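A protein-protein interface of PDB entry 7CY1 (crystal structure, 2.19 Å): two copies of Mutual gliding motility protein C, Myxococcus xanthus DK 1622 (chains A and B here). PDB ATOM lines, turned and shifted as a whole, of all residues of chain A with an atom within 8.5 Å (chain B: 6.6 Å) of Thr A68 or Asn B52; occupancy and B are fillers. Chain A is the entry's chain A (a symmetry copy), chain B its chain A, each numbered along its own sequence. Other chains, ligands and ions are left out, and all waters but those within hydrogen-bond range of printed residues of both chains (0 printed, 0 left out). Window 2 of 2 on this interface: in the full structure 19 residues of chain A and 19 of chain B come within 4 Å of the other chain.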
ATOM      1  N   THR A  63      -1.778  16.578 -19.054  1.00  0.00           N
ATOM      2  CA  THR A  63      -1.611  18.010 -18.685  1.00  0.00           C
ATOM      3  C   THR A  63      -2.885  18.811 -19.015  1.00  0.00           C
ATOM      4  O   THR A  63      -3.040  19.895 -18.428  1.00  0.00           O
ATOM      5  CB  THR A  63      -0.374  18.652 -19.327  1.00  0.00           C
ATOM      6  OG1 THR A  63      -0.637  18.900 -20.701  1.00  0.00           O
ATOM      7  CG2 THR A  63       0.884  17.826 -19.178  1.00  0.00           C
ATOM      8  N   LEU A  64      -3.758  18.335 -19.909  1.00  0.00           N
ATOM      9  CA  LEU A  64      -5.040  19.023 -20.247  1.00  0.00           C
ATOM     10  C   LEU A  64      -5.946  19.130 -19.017  1.00  0.00           C
ATOM     11  O   LEU A  64      -6.789  20.025 -18.994  1.00  0.00           O
ATOM     12  CB  LEU A  64      -5.783  18.250 -21.337  1.00  0.00           C
ATOM     13  CG  LEU A  64      -5.188  18.341 -22.740  1.00  0.00           C
ATOM     14  CD1 LEU A  64      -5.866  17.341 -23.670  1.00  0.00           C
ATOM     15  CD2 LEU A  64      -5.314  19.754 -23.270  1.00  0.00           C
ATOM     16  N   LYS A  65      -5.806  18.245 -18.040  1.00  0.00           N
ATOM     17  CA  LYS A  65      -6.688  18.226 -16.844  1.00  0.00           C
ATOM     18  C   LYS A  65      -6.430  19.436 -15.935  1.00  0.00           C
ATOM     19  O   LYS A  65      -7.337  19.796 -15.199  1.00  0.00           O
ATOM     20  CB  LYS A  65      -6.486  16.930 -16.070  1.00  0.00           C
ATOM     21  CG  LYS A  65      -7.181  15.729 -16.676  1.00  0.00           C
ATOM     22  CD  LYS A  65      -6.511  14.460 -16.243  1.00  0.00           C
ATOM     23  CE  LYS A  65      -7.481  13.313 -16.126  1.00  0.00           C
ATOM     24  NZ  LYS A  65      -6.743  12.042 -15.941  1.00  0.00           N
ATOM     25  N   THR A  66      -5.254  20.054 -15.978  1.00  0.00           N
ATOM     26  CA  THR A  66      -4.978  21.274 -15.178  1.00  0.00           C
ATOM     27  C   THR A  66      -5.783  22.451 -15.753  1.00  0.00           C
ATOM     28  O   THR A  66      -6.113  22.426 -16.970  1.00  0.00           O
ATOM     29  CB  THR A  66      -3.481  21.581 -15.151  1.00  0.00           C
ATOM     30  OG1 THR A  66      -3.146  22.030 -16.465  1.00  0.00           O
ATOM     31  CG2 THR A  66      -2.644  20.385 -14.748  1.00  0.00           C
ATOM     32  N   GLY A  67      -6.067  23.456 -14.923  1.00  0.00           N
ATOM     33  CA  GLY A  67      -6.864  24.635 -15.316  1.00  0.00           C
ATOM     34  C   GLY A  67      -6.186  25.466 -16.390  1.00  0.00           C
ATOM     35  O   GLY A  67      -6.884  25.926 -17.307  1.00  0.00           O
ATOM     36  N   THR A  68      -4.866  25.624 -16.322  1.00  0.00           N
ATOM     37  CA  THR A  68      -4.115  26.534 -17.230  1.00  0.00           C
ATOM     38  C   THR A  68      -4.035  25.962 -18.652  1.00  0.00           C
ATOM     39  O   THR A  68      -4.054  26.757 -19.621  1.00  0.00           O
ATOM     40  CB  THR A  68      -2.704  26.788 -16.702  1.00  0.00           C
ATOM     41  OG1 THR A  68      -2.828  26.986 -15.298  1.00  0.00           O
ATOM     42  CG2 THR A  68      -2.046  27.990 -17.343  1.00  0.00           C
ATOM     43  N   VAL A  69      -3.861  24.650 -18.787  1.00  0.00           N
ATOM     44  CA  VAL A  69      -3.538  24.025 -20.106  1.00  0.00           C
ATOM     45  C   VAL A  69      -4.842  23.813 -20.874  1.00  0.00           C
ATOM     46  O   VAL A  69      -5.698  23.091 -20.349  1.00  0.00           O
ATOM     47  CB  VAL A  69      -2.801  22.696 -19.909  1.00  0.00           C
ATOM     48  CG1 VAL A  69      -2.491  22.034 -21.243  1.00  0.00           C
ATOM     49  CG2 VAL A  69      -1.538  22.894 -19.096  1.00  0.00           C
ATOM     50  N   SER A  70      -5.004  24.416 -22.050  1.00  0.00           N
ATOM     51  CA  SER A  70      -6.227  24.216 -22.871  1.00  0.00           C
ATOM     52  C   SER A  70      -5.966  23.392 -24.153  1.00  0.00           C
ATOM     53  O   SER A  70      -6.946  22.844 -24.688  1.00  0.00           O
ATOM     54  CB  SER A  70      -6.880  25.547 -23.159  1.00  0.00           C
ATOM     55  OG  SER A  70      -5.913  26.482 -23.583  1.00  0.00           O
ATOM     56  N   GLU A  71      -4.713  23.243 -24.591  1.00  0.00           N
ATOM     57  CA  GLU A  71      -4.336  22.643 -25.899  1.00  0.00           C
ATOM     58  C   GLU A  71      -2.923  22.038 -25.792  1.00  0.00           C
ATOM     59  O   GLU A  71      -2.010  22.712 -25.266  1.00  0.00           O
ATOM     60  CB  GLU A  71      -4.477  23.758 -26.941  1.00  0.00           C
ATOM     61  CG  GLU A  71      -4.220  23.379 -28.385  1.00  0.00           C
ATOM     62  CD  GLU A  71      -4.120  24.625 -29.267  1.00  0.00           C
ATOM     63  OE1 GLU A  71      -3.149  25.394 -29.100  1.00  0.00           O
ATOM     64  OE2 GLU A  71      -5.034  24.865 -30.086  1.00  0.00           O
ATOM     65  N   TRP B  47       2.645  36.215 -18.483  1.00  0.00           N
ATOM     66  CA  TRP B  47       3.643  35.799 -17.461  1.00  0.00           C
ATOM     67  C   TRP B  47       2.982  34.953 -16.377  1.00  0.00           C
ATOM     68  O   TRP B  47       3.540  33.930 -16.028  1.00  0.00           O
ATOM     69  CB  TRP B  47       4.336  37.024 -16.873  1.00  0.00           C
ATOM     70  CG  TRP B  47       5.237  37.682 -17.868  1.00  0.00           C
ATOM     71  CD1 TRP B  47       5.176  38.972 -18.307  1.00  0.00           C
ATOM     72  CD2 TRP B  47       6.340  37.074 -18.553  1.00  0.00           C
ATOM     73  NE1 TRP B  47       6.174  39.210 -19.209  1.00  0.00           N
ATOM     74  CE2 TRP B  47       6.907  38.066 -19.380  1.00  0.00           C
ATOM     75  CE3 TRP B  47       6.924  35.807 -18.523  1.00  0.00           C
ATOM     76  CZ2 TRP B  47       8.010  37.822 -20.192  1.00  0.00           C
ATOM     77  CZ3 TRP B  47       8.018  35.567 -19.323  1.00  0.00           C
ATOM     78  CH2 TRP B  47       8.555  36.562 -20.139  1.00  0.00           C
ATOM     79  N   VAL B  48       1.818  35.353 -15.870  1.00  0.00           N
ATOM     80  CA  VAL B  48       1.101  34.536 -14.859  1.00  0.00           C
ATOM     81  C   VAL B  48       0.881  33.133 -15.443  1.00  0.00           C
ATOM     82  O   VAL B  48       1.240  32.158 -14.784  1.00  0.00           O
ATOM     83  CB  VAL B  48      -0.216  35.199 -14.421  1.00  0.00           C
ATOM     84  CG1 VAL B  48      -1.113  34.227 -13.666  1.00  0.00           C
ATOM     85  CG2 VAL B  48       0.060  36.439 -13.590  1.00  0.00           C
ATOM     86  N   GLU B  49       0.295  33.022 -16.635  1.00  0.00           N
ATOM     87  CA  GLU B  49      -0.025  31.700 -17.241  1.00  0.00           C
ATOM     88  C   GLU B  49       1.269  30.957 -17.576  1.00  0.00           C
ATOM     89  O   GLU B  49       1.281  29.738 -17.386  1.00  0.00           O
ATOM     90  CB  GLU B  49      -0.883  31.843 -18.487  1.00  0.00           C
ATOM     91  CG  GLU B  49      -2.267  32.343 -18.154  1.00  0.00           C
ATOM     92  CD  GLU B  49      -3.290  32.043 -19.229  1.00  0.00           C
ATOM     93  OE1 GLU B  49      -2.875  31.762 -20.368  1.00  0.00           O
ATOM     94  OE2 GLU B  49      -4.494  32.090 -18.921  1.00  0.00           O
ATOM     95  N   TYR B  50       2.320  31.664 -17.993  1.00  0.00           N
ATOM     96  CA  TYR B  50       3.644  31.059 -18.266  1.00  0.00           C
ATOM     97  C   TYR B  50       4.186  30.381 -16.997  1.00  0.00           C
ATOM     98  O   TYR B  50       4.656  29.239 -17.085  1.00  0.00           O
ATOM     99  CB  TYR B  50       4.633  32.085 -18.812  1.00  0.00           C
ATOM    100  CG  TYR B  50       5.932  31.457 -19.256  1.00  0.00           C
ATOM    101  CD1 TYR B  50       5.963  30.176 -19.789  1.00  0.00           C
ATOM    102  CD2 TYR B  50       7.135  32.125 -19.119  1.00  0.00           C
ATOM    103  CE1 TYR B  50       7.148  29.584 -20.189  1.00  0.00           C
ATOM    104  CE2 TYR B  50       8.331  31.548 -19.515  1.00  0.00           C
ATOM    105  CZ  TYR B  50       8.333  30.277 -20.056  1.00  0.00           C
ATOM    106  OH  TYR B  50       9.499  29.699 -20.455  1.00  0.00           O
ATOM    107  N   ALA B  51       4.107  31.051 -15.844  1.00  0.00           N
ATOM    108  CA  ALA B  51       4.576  30.517 -14.545  1.00  0.00           C
ATOM    109  C   ALA B  51       3.750  29.282 -14.200  1.00  0.00           C
ATOM    110  O   ALA B  51       4.313  28.305 -13.743  1.00  0.00           O
ATOM    111  CB  ALA B  51       4.463  31.570 -13.467  1.00  0.00           C
ATOM    112  N   ASN B  52       2.453  29.341 -14.453  1.00  0.00           N
ATOM    113  CA  ASN B  52       1.499  28.249 -14.164  1.00  0.00           C
ATOM    114  C   ASN B  52       1.730  27.082 -15.140  1.00  0.00           C
ATOM    115  O   ASN B  52       1.350  25.964 -14.785  1.00  0.00           O
ATOM    116  CB  ASN B  52       0.060  28.780 -14.163  1.00  0.00           C
ATOM    117  CG  ASN B  52      -0.213  29.679 -12.968  1.00  0.00           C
ATOM    118  OD1 ASN B  52       0.510  29.634 -11.978  1.00  0.00           O
ATOM    119  ND2 ASN B  52      -1.212  30.537 -13.062  1.00  0.00           N
ATOM    120  N   LEU B  53       2.333  27.304 -16.312  1.00  0.00           N
ATOM    121  CA  LEU B  53       2.550  26.207 -17.294  1.00  0.00           C
ATOM    122  C   LEU B  53       3.787  25.381 -16.919  1.00  0.00           C
ATOM    123  O   LEU B  53       3.846  24.246 -17.381  1.00  0.00           O
ATOM    124  CB  LEU B  53       2.698  26.769 -18.713  1.00  0.00           C
ATOM    125  CG  LEU B  53       1.406  27.177 -19.412  1.00  0.00           C
ATOM    126  CD1 LEU B  53       1.709  27.808 -20.759  1.00  0.00           C
ATOM    127  CD2 LEU B  53       0.457  26.004 -19.575  1.00  0.00           C
ATOM    128  N   LEU B  54       4.711  25.893 -16.101  1.00  0.00           N
ATOM    129  CA  LEU B  54       6.083  25.311 -15.990  1.00  0.00           C
ATOM    130  C   LEU B  54       6.067  23.843 -15.537  1.00  0.00           C
ATOM    131  O   LEU B  54       6.881  23.076 -16.084  1.00  0.00           O
ATOM    132  CB  LEU B  54       6.969  26.154 -15.076  1.00  0.00           C
ATOM    133  CG  LEU B  54       7.397  27.515 -15.620  1.00  0.00           C
ATOM    134  CD1 LEU B  54       8.248  28.234 -14.587  1.00  0.00           C
ATOM    135  CD2 LEU B  54       8.139  27.412 -16.947  1.00  0.00           C
ATOM    136  N   THR B  55       5.213  23.423 -14.603  1.00  0.00           N
ATOM    137  CA  THR B  55       5.180  21.997 -14.176  1.00  0.00           C
ATOM    138  C   THR B  55       4.746  21.114 -15.347  1.00  0.00           C
ATOM    139  O   THR B  55       5.336  20.007 -15.565  1.00  0.00           O
ATOM    140  CB  THR B  55       4.174  21.732 -13.050  1.00  0.00           C
ATOM    141  OG1 THR B  55       4.428  22.716 -12.052  1.00  0.00           O
ATOM    142  CG2 THR B  55       4.267  20.331 -12.478  1.00  0.00           C
ATOM    143  N   GLN B  56       3.714  21.574 -16.047  1.00  0.00           N
ATOM    144  CA  GLN B  56       3.064  20.817 -17.146  1.00  0.00           C
ATOM    145  C   GLN B  56       4.055  20.695 -18.313  1.00  0.00           C
ATOM    146  O   GLN B  56       4.095  19.632 -18.948  1.00  0.00           O
ATOM    147  CB  GLN B  56       1.749  21.511 -17.512  1.00  0.00           C
ATOM    148  CG  GLN B  56       0.822  21.753 -16.327  1.00  0.00           C
ATOM    149  CD  GLN B  56       0.876  20.612 -15.343  1.00  0.00           C
ATOM    150  OE1 GLN B  56       1.300  20.792 -14.209  1.00  0.00           O
ATOM    151  NE2 GLN B  56       0.491  19.420 -15.785  1.00  0.00           N
ATOM    152  N   ASN B  75      -0.090  24.599 -24.275  1.00  0.00           N
ATOM    153  CA  ASN B  75      -0.622  25.950 -24.554  1.00  0.00           C
ATOM    154  C   ASN B  75      -1.766  26.250 -23.600  1.00  0.00           C
ATOM    155  O   ASN B  75      -2.518  25.323 -23.226  1.00  0.00           O
ATOM    156  CB  ASN B  75      -1.174  26.109 -25.967  1.00  0.00           C
ATOM    157  CG  ASN B  75      -0.119  25.967 -27.032  1.00  0.00           C
ATOM    158  OD1 ASN B  75       1.070  25.990 -26.732  1.00  0.00           O
ATOM    159  ND2 ASN B  75      -0.559  25.809 -28.266  1.00  0.00           N
ATOM    160  N   SER B  76      -1.882  27.525 -23.259  1.00  0.00           N
ATOM    161  CA  SER B  76      -2.994  28.083 -22.460  1.00  0.00           C
ATOM    162  C   SER B  76      -3.749  29.076 -23.341  1.00  0.00           C
ATOM    163  O   SER B  76      -3.386  29.208 -24.525  1.00  0.00           O
ATOM    164  CB  SER B  76      -2.453  28.731 -21.230  1.00  0.00           C
ATOM    165  OG  SER B  76      -1.690  29.876 -21.578  1.00  0.00           O
ATOM    166  N   GLU B  77      -4.730  29.762 -22.769  1.00  0.00           N
ATOM    167  CA  GLU B  77      -5.497  30.812 -23.473  1.00  0.00           C
ATOM    168  C   GLU B  77      -4.531  31.918 -23.916  1.00  0.00           C
ATOM    169  O   GLU B  77      -4.674  32.352 -25.043  1.00  0.00           O
ATOM    170  CB  GLU B  77      -6.635  31.338 -22.594  1.00  0.00           C
ATOM    171  CG  GLU B  77      -7.795  31.887 -23.412  1.00  0.00           C
ATOM    172  CD  GLU B  77      -9.078  32.182 -22.645  1.00  0.00           C
ATOM    173  OE1 GLU B  77      -8.984  32.747 -21.532  1.00  0.00           O
ATOM    174  OE2 GLU B  77     -10.176  31.853 -23.167  1.00  0.00           O
ATOM    175  N   LYS B  78      -3.559  32.319 -23.084  1.00  0.00           N
ATOM    176  CA  LYS B  78      -2.680  33.500 -23.349  1.00  0.00           C
ATOM    177  C   LYS B  78      -1.267  33.123 -23.813  1.00  0.00           C
ATOM    178  O   LYS B  78      -0.601  33.999 -24.402  1.00  0.00           O
ATOM    179  CB  LYS B  78      -2.537  34.375 -22.104  1.00  0.00           C
ATOM    180  CG  LYS B  78      -3.772  35.183 -21.763  1.00  0.00           C
ATOM    181  CD  LYS B  78      -3.824  35.582 -20.317  1.00  0.00           C
ATOM    182  CE  LYS B  78      -4.840  36.668 -20.053  1.00  0.00           C
ATOM    183  NZ  LYS B  78      -5.258  36.674 -18.633  1.00  0.00           N
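ND2 of Asn B52 lies close to O of Val B48 (3.4 Å).
The side-chain carboxylate (OE1) of Glu B49 lies within hydrogen-bond range of the side-chain hydroxyl (OG) of Ser B76 (2.5 Å).
OE1 of Glu B49 sits at hydrogen-bond distance from N of Lys B78, 2.9 Å away.
OG of Ser B76 sits close to N of Lys B78, 3.4 Å away.
O of Thr A63 is in hydrogen-bond range of OG1 of Thr A66.
No position is printed for both chains.
Of the 13 pairs that touch across the chains among the printed residues, none has its exchanged pair printed and touching as well.
Among the printed residues, merely in contact across the chains: Thr A63 with Gln B56 (3.7 Å), Thr A66 with Gln B56 (3.4 Å), Thr A68 with Glu B49 (3.8 Å), Thr A68 with Asn B52 (3.6 Å), Thr A68 with Leu B53 (3.9 Å), Thr A68 with Ser B76 (3.0 Å), Val A69 with Leu B53 (3.7 Å), Val A69 with Gln B56 (3.8 Å), Val A69 with Asn B75 (3.5 Å), Ser A70 with Ser B76 (3.4 Å) and Ser A70 with Glu B77 (3.6 Å).
Of the 14 printed residues of chain B, 7 touch a printed residue of chain A.
Along chain B the printed residues that touch a printed residue of chain A span positions 49 to 77.
Of the 9 printed residues of chain A, 6 touch a printed residue of chain B.
Hydrophobic or aromatic side chains of chain A within 4 Å of the printed part of chain B: Val A69.
Among the printed residues, no Asp or Glu carboxylate lies within 4 Å of a Lys or Arg side-chain nitrogen of the other chain.
O of Asn B75 is in hydrogen-bond range of N of Ser A70, at 2.9 Å.
ND2 of Asn B75 lies within hydrogen-bond range of OE1 of Glu A71 (2.8 Å).
Thr A68 touches four residues of chain B.
Printed residues of chain B within 4 Å of Val A69: Leu B53 (3.7 Å), Gln B56 (3.8 Å) and Asn B75 (3.5 Å).
No residue of chain A comes within 4 Å of Ala B51.
Of the printed residues of chain A, Asn B52 touches Thr A68 (3.6 Å).
Of the printed residues of chain A, Glu B77 touches Ser A70.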
